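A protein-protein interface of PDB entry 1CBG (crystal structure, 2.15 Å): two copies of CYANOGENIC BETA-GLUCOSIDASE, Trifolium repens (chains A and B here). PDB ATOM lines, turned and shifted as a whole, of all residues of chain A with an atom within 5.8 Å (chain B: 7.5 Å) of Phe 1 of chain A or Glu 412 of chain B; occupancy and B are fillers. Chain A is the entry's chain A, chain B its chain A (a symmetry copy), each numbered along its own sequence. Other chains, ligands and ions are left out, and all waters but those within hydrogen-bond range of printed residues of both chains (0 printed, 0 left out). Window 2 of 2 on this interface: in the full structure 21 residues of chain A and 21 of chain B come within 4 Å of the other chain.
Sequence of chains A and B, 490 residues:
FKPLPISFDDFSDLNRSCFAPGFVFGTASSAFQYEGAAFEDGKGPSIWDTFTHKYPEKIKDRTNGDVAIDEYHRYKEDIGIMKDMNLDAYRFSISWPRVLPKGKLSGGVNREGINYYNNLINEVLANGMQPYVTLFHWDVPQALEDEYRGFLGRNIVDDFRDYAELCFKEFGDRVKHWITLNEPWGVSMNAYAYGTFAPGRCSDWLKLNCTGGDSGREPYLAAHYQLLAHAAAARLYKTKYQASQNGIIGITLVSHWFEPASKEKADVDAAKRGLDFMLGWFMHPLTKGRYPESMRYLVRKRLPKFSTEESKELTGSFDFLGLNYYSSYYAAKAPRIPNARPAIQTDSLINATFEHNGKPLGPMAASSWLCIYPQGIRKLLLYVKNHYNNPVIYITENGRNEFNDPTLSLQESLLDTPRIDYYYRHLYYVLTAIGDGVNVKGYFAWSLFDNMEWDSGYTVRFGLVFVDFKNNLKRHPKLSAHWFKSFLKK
Glu 412 of chain B touches three residues of chain A.
Printed residues of chain A within 4 Å of Gln 411 of chain B: Pro 3 (3.2 Å) and Tyr 428 (2.7 Å).
Printed residues of chain A within 4 Å of Leu 415 of chain B: Tyr 428 (3.4 Å).
Printed residues of chain B within 4 Å of Pro 3 of chain A: Gln 411 (3.2 Å).
Printed residues of chain B within 4 Å of Tyr 428 of chain A: Gln 411 (2.7 Å), Glu 412 (3.9 Å) and Leu 415 (3.4 Å).
Lys 2 of chain A touches none of the printed residues of chain B.
The nearest residue of chain A that does not touch Glu 412 of chain B is Gln 375 of chain A (4.5 Å).
Of the 10 printed residues of chain B, 4 touch a printed residue of chain A.
Hydrophobic or aromatic side chains of chain B that line the printed part of chain A: Leu 415.
Along chain A the printed residues that touch a printed residue of chain B span positions 1 to 429.
Among the printed residues, 7 pairs touch across the chains.
Among the printed residues, no Asp or Glu carboxylate lies within 4 Å of a Lys or Arg side-chain nitrogen of the other chain.
Among the printed residues, merely in contact across the chains: Phe 1 of chain A with Ser 409 of chain B (3.9 Å), Phe 1 of chain A with Glu 412 of chain B (3.5 Å), Pro 3 of chain A with Gln 411 of chain B (3.2 Å), Tyr 428 of chain A with Glu 412 of chain B (3.9 Å) and Tyr 428 of chain A with Leu 415 of chain B (3.4 Å).
OH of Tyr 428 of chain A lies within hydrogen-bond range of OE1 of Gln 411 of chain B, 2.7 Å away.
The side-chain carboxylate (OE2) of Glu 412 of chain B sits at hydrogen-bond distance from the side-chain hydroxyl (OH) of Tyr 429 of chain A (2.6 Å).
No position is printed for both chains.
Of the 7 pairs that touch across the chains among the printed residues, none has its exchanged pair printed and touching as well.
The side-chain hydroxyl of Ser 409 of chain B is in hydrogen-bond range of the side-chain carboxylate of Glu 412 of chain B.
The backbone carbonyl oxygen (O) of Tyr 429 of chain A is in hydrogen-bond range of the side-chain hydroxyl (OG1) of Thr 432 of chain A.
The backbone carbonyl oxygen (O) of Ser 409 of chain B is in hydrogen-bond range of the side-chain hydroxyl (OG) of Ser 413 of chain B (3.4 Å).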
ATOM      1  N   PHE A   1      20.706   2.389  26.129  1.00  0.00           N
ATOM      2  CA  PHE A   1      22.122   2.351  25.718  1.00  0.00           C
ATOM      3  C   PHE A   1      22.974   1.937  26.924  1.00  0.00           C
ATOM      4  O   PHE A   1      22.738   2.365  28.066  1.00  0.00           O
ATOM      5  CB  PHE A   1      22.584   3.687  25.156  1.00  0.00           C
ATOM      6  CG  PHE A   1      23.798   3.765  24.291  1.00  0.00           C
ATOM      7  CD1 PHE A   1      25.073   3.510  24.787  1.00  0.00           C
ATOM      8  CD2 PHE A   1      23.672   4.133  22.953  1.00  0.00           C
ATOM      9  CE1 PHE A   1      26.213   3.578  23.980  1.00  0.00           C
ATOM     10  CE2 PHE A   1      24.776   4.213  22.123  1.00  0.00           C
ATOM     11  CZ  PHE A   1      26.046   3.934  22.633  1.00  0.00           C
ATOM     12  N   LYS A   2      23.943   1.111  26.603  1.00  0.00           N
ATOM     13  CA  LYS A   2      24.960   0.606  27.544  1.00  0.00           C
ATOM     14  C   LYS A   2      26.170   0.334  26.623  1.00  0.00           C
ATOM     15  O   LYS A   2      26.072  -0.343  25.587  1.00  0.00           O
ATOM     16  CB  LYS A   2      24.567  -0.560  28.415  1.00  0.00           C
ATOM     17  CG  LYS A   2      25.070  -0.459  29.872  1.00  0.00           C
ATOM     18  CD  LYS A   2      24.257   0.559  30.662  1.00  0.00           C
ATOM     19  CE  LYS A   2      25.021   1.287  31.745  1.00  0.00           C
ATOM     20  NZ  LYS A   2      24.467   2.657  31.968  1.00  0.00           N
ATOM     21  N   PRO A   3      27.278   0.950  27.028  1.00  0.00           N
ATOM     22  CA  PRO A   3      28.539   0.888  26.291  1.00  0.00           C
ATOM     23  C   PRO A   3      29.078  -0.508  26.020  1.00  0.00           C
ATOM     24  O   PRO A   3      28.513  -1.547  26.392  1.00  0.00           O
ATOM     25  CB  PRO A   3      29.508   1.751  27.104  1.00  0.00           C
ATOM     26  CG  PRO A   3      28.919   1.903  28.473  1.00  0.00           C
ATOM     27  CD  PRO A   3      27.414   1.787  28.234  1.00  0.00           C
ATOM     28  N   GLN A 375      24.619   8.226  15.157  1.00  0.00           N
ATOM     29  CA  GLN A 375      23.614   7.693  16.048  1.00  0.00           C
ATOM     30  C   GLN A 375      22.405   7.166  15.256  1.00  0.00           C
ATOM     31  O   GLN A 375      21.782   6.192  15.714  1.00  0.00           O
ATOM     32  CB  GLN A 375      23.082   8.677  17.108  1.00  0.00           C
ATOM     33  CG  GLN A 375      24.164   9.274  17.970  1.00  0.00           C
ATOM     34  CD  GLN A 375      24.473  10.711  17.614  1.00  0.00           C
ATOM     35  OE1 GLN A 375      24.040  11.565  18.399  1.00  0.00           O
ATOM     36  NE2 GLN A 375      25.180  10.973  16.510  1.00  0.00           N
ATOM     37  N   ARG A 378      22.349   3.306  14.409  1.00  0.00           N
ATOM     38  CA  ARG A 378      21.971   2.520  15.583  1.00  0.00           C
ATOM     39  C   ARG A 378      20.470   2.618  15.825  1.00  0.00           C
ATOM     40  O   ARG A 378      19.814   1.579  16.020  1.00  0.00           O
ATOM     41  CB  ARG A 378      22.776   2.913  16.828  1.00  0.00           C
ATOM     42  CG  ARG A 378      22.312   2.236  18.109  1.00  0.00           C
ATOM     43  CD  ARG A 378      22.720   3.022  19.318  1.00  0.00           C
ATOM     44  NE  ARG A 378      21.822   2.777  20.440  1.00  0.00           N
ATOM     45  CZ  ARG A 378      21.877   1.717  21.240  1.00  0.00           C
ATOM     46  NH1 ARG A 378      22.796   0.768  21.097  1.00  0.00           N
ATOM     47  NH2 ARG A 378      21.009   1.583  22.249  1.00  0.00           N
ATOM     48  N   TYR A 428      31.307   2.057  14.966  1.00  0.00           N
ATOM     49  CA  TYR A 428      31.134   2.002  16.417  1.00  0.00           C
ATOM     50  C   TYR A 428      29.643   1.817  16.715  1.00  0.00           C
ATOM     51  O   TYR A 428      29.307   0.971  17.557  1.00  0.00           O
ATOM     52  CB  TYR A 428      31.730   3.232  17.144  1.00  0.00           C
ATOM     53  CG  TYR A 428      31.227   3.375  18.573  1.00  0.00           C
ATOM     54  CD1 TYR A 428      31.813   2.646  19.611  1.00  0.00           C
ATOM     55  CD2 TYR A 428      30.139   4.194  18.868  1.00  0.00           C
ATOM     56  CE1 TYR A 428      31.327   2.754  20.912  1.00  0.00           C
ATOM     57  CE2 TYR A 428      29.647   4.313  20.162  1.00  0.00           C
ATOM     58  CZ  TYR A 428      30.251   3.586  21.182  1.00  0.00           C
ATOM     59  OH  TYR A 428      29.752   3.710  22.455  1.00  0.00           O
ATOM     60  N   TYR A 429      28.742   2.571  16.116  1.00  0.00           N
ATOM     61  CA  TYR A 429      27.302   2.486  16.380  1.00  0.00           C
ATOM     62  C   TYR A 429      26.653   1.189  15.909  1.00  0.00           C
ATOM     63  O   TYR A 429      25.712   0.679  16.565  1.00  0.00           O
ATOM     64  CB  TYR A 429      26.555   3.755  15.927  1.00  0.00           C
ATOM     65  CG  TYR A 429      26.696   4.889  16.927  1.00  0.00           C
ATOM     66  CD1 TYR A 429      26.013   4.862  18.148  1.00  0.00           C
ATOM     67  CD2 TYR A 429      27.507   5.987  16.666  1.00  0.00           C
ATOM     68  CE1 TYR A 429      26.125   5.894  19.075  1.00  0.00           C
ATOM     69  CE2 TYR A 429      27.627   7.039  17.567  1.00  0.00           C
ATOM     70  CZ  TYR A 429      26.937   6.988  18.777  1.00  0.00           C
ATOM     71  OH  TYR A 429      27.032   7.994  19.697  1.00  0.00           O
ATOM     72  N   THR A 432      27.275  -1.236  18.684  1.00  0.00           N
ATOM     73  CA  THR A 432      26.363  -1.026  19.809  1.00  0.00           C
ATOM     74  C   THR A 432      24.990  -1.610  19.486  1.00  0.00           C
ATOM     75  O   THR A 432      24.368  -2.119  20.439  1.00  0.00           O
ATOM     76  CB  THR A 432      26.279   0.460  20.335  1.00  0.00           C
ATOM     77  OG1 THR A 432      25.534   1.250  19.365  1.00  0.00           O
ATOM     78  CG2 THR A 432      27.640   1.117  20.627  1.00  0.00           C
ATOM     79  N   ASP A 436      22.909  -4.766  21.558  1.00  0.00           N
ATOM     80  CA  ASP A 436      21.510  -4.672  21.933  1.00  0.00           C
ATOM     81  C   ASP A 436      20.552  -5.634  21.233  1.00  0.00           C
ATOM     82  O   ASP A 436      19.320  -5.457  21.318  1.00  0.00           O
ATOM     83  CB  ASP A 436      21.064  -3.204  21.785  1.00  0.00           C
ATOM     84  CG  ASP A 436      21.744  -2.373  22.868  1.00  0.00           C
ATOM     85  OD1 ASP A 436      22.155  -2.862  23.933  1.00  0.00           O
ATOM     86  OD2 ASP A 436      21.890  -1.167  22.620  1.00  0.00           O
ATOM     87  N   THR B 407      22.648  13.847  26.655  1.00  0.00           N
ATOM     88  CA  THR B 407      22.063  12.569  26.292  1.00  0.00           C
ATOM     89  C   THR B 407      23.138  11.556  25.921  1.00  0.00           C
ATOM     90  O   THR B 407      22.785  10.364  25.943  1.00  0.00           O
ATOM     91  CB  THR B 407      21.012  12.733  25.134  1.00  0.00           C
ATOM     92  OG1 THR B 407      21.800  13.030  23.932  1.00  0.00           O
ATOM     93  CG2 THR B 407      19.969  13.820  25.414  1.00  0.00           C
ATOM     94  N   LEU B 408      24.358  11.965  25.611  1.00  0.00           N
ATOM     95  CA  LEU B 408      25.448  11.050  25.276  1.00  0.00           C
ATOM     96  C   LEU B 408      26.118  10.455  26.519  1.00  0.00           C
ATOM     97  O   LEU B 408      26.317  11.158  27.514  1.00  0.00           O
ATOM     98  CB  LEU B 408      26.489  11.791  24.425  1.00  0.00           C
ATOM     99  CG  LEU B 408      26.149  12.351  23.073  1.00  0.00           C
ATOM    100  CD1 LEU B 408      27.395  13.005  22.470  1.00  0.00           C
ATOM    101  CD2 LEU B 408      25.677  11.255  22.116  1.00  0.00           C
ATOM    102  N   SER B 409      26.468   9.182  26.424  1.00  0.00           N
ATOM    103  CA  SER B 409      27.178   8.452  27.475  1.00  0.00           C
ATOM    104  C   SER B 409      28.629   8.940  27.418  1.00  0.00           C
ATOM    105  O   SER B 409      29.020   9.583  26.423  1.00  0.00           O
ATOM    106  CB  SER B 409      27.113   6.944  27.291  1.00  0.00           C
ATOM    107  OG  SER B 409      27.662   6.521  26.048  1.00  0.00           O
ATOM    108  N   LEU B 410      29.435   8.606  28.409  1.00  0.00           N
ATOM    109  CA  LEU B 410      30.845   9.013  28.441  1.00  0.00           C
ATOM    110  C   LEU B 410      31.620   8.458  27.264  1.00  0.00           C
ATOM    111  O   LEU B 410      32.323   9.225  26.573  1.00  0.00           O
ATOM    112  CB  LEU B 410      31.528   8.700  29.792  1.00  0.00           C
ATOM    113  CG  LEU B 410      33.010   9.093  29.863  1.00  0.00           C
ATOM    114  CD1 LEU B 410      33.204  10.604  29.872  1.00  0.00           C
ATOM    115  CD2 LEU B 410      33.649   8.497  31.122  1.00  0.00           C
ATOM    116  N   GLN B 411      31.519   7.168  26.992  1.00  0.00           N
ATOM    117  CA  GLN B 411      32.194   6.467  25.874  1.00  0.00           C
ATOM    118  C   GLN B 411      31.944   7.139  24.526  1.00  0.00           C
ATOM    119  O   GLN B 411      32.869   7.353  23.718  1.00  0.00           O
ATOM    120  CB  GLN B 411      31.792   4.987  25.868  1.00  0.00           C
ATOM    121  CG  GLN B 411      32.526   4.123  24.854  1.00  0.00           C
ATOM    122  CD  GLN B 411      32.060   2.680  24.890  1.00  0.00           C
ATOM    123  OE1 GLN B 411      31.016   2.283  24.362  1.00  0.00           O
ATOM    124  NE2 GLN B 411      32.890   1.885  25.558  1.00  0.00           N
ATOM    125  N   GLU B 412      30.718   7.530  24.240  1.00  0.00           N
ATOM    126  CA  GLU B 412      30.238   8.236  23.063  1.00  0.00           C
ATOM    127  C   GLU B 412      30.839   9.629  22.963  1.00  0.00           C
ATOM    128  O   GLU B 412      31.240  10.098  21.890  1.00  0.00           O
ATOM    129  CB  GLU B 412      28.714   8.390  23.051  1.00  0.00           C
ATOM    130  CG  GLU B 412      27.886   7.116  22.763  1.00  0.00           C
ATOM    131  CD  GLU B 412      26.408   7.388  22.860  1.00  0.00           C
ATOM    132  OE1 GLU B 412      26.046   7.400  24.056  1.00  0.00           O
ATOM    133  OE2 GLU B 412      25.707   7.574  21.885  1.00  0.00           O
ATOM    134  N   SER B 413      30.950  10.308  24.095  1.00  0.00           N
ATOM    135  CA  SER B 413      31.550  11.646  24.233  1.00  0.00           C
ATOM    136  C   SER B 413      33.052  11.622  23.975  1.00  0.00           C
ATOM    137  O   SER B 413      33.601  12.611  23.449  1.00  0.00           O
ATOM    138  CB  SER B 413      31.211  12.231  25.606  1.00  0.00           C
ATOM    139  OG  SER B 413      29.900  12.770  25.646  1.00  0.00           O
ATOM    140  N   LEU B 414      33.766  10.554  24.280  1.00  0.00           N
ATOM    141  CA  LEU B 414      35.197  10.409  24.049  1.00  0.00           C
ATOM    142  C   LEU B 414      35.566  10.052  22.613  1.00  0.00           C
ATOM    143  O   LEU B 414      36.778  10.164  22.267  1.00  0.00           O
ATOM    144  CB  LEU B 414      35.770   9.438  25.101  1.00  0.00           C
ATOM    145  CG  LEU B 414      35.558   9.676  26.584  1.00  0.00           C
ATOM    146  CD1 LEU B 414      36.341   8.654  27.417  1.00  0.00           C
ATOM    147  CD2 LEU B 414      36.020  11.080  26.988  1.00  0.00           C
ATOM    148  N   LEU B 415      34.655   9.674  21.731  1.00  0.00           N
ATOM    149  CA  LEU B 415      34.966   9.325  20.336  1.00  0.00           C
ATOM    150  C   LEU B 415      34.934  10.540  19.403  1.00  0.00           C
ATOM    151  O   LEU B 415      34.082  10.666  18.503  1.00  0.00           O
ATOM    152  CB  LEU B 415      34.020   8.224  19.861  1.00  0.00           C
ATOM    153  CG  LEU B 415      34.029   6.787  20.267  1.00  0.00           C
ATOM    154  CD1 LEU B 415      33.358   5.992  19.126  1.00  0.00           C
ATOM    155  CD2 LEU B 415      35.418   6.194  20.484  1.00  0.00           C
ATOM    156  N   ASP B 416      35.897  11.423  19.575  1.00  0.00           N
ATOM    157  CA  ASP B 416      36.067  12.684  18.859  1.00  0.00           C
ATOM    158  C   ASP B 416      36.983  12.577  17.648  1.00  0.00           C
ATOM    159  O   ASP B 416      37.944  13.316  17.418  1.00  0.00           O
ATOM    160  CB  ASP B 416      36.465  13.807  19.848  1.00  0.00           C
ATOM    161  CG  ASP B 416      37.897  13.774  20.351  1.00  0.00           C
ATOM    162  OD1 ASP B 416      38.544  12.708  20.336  1.00  0.00           O
ATOM    163  OD2 ASP B 416      38.412  14.854  20.703  1.00  0.00           O
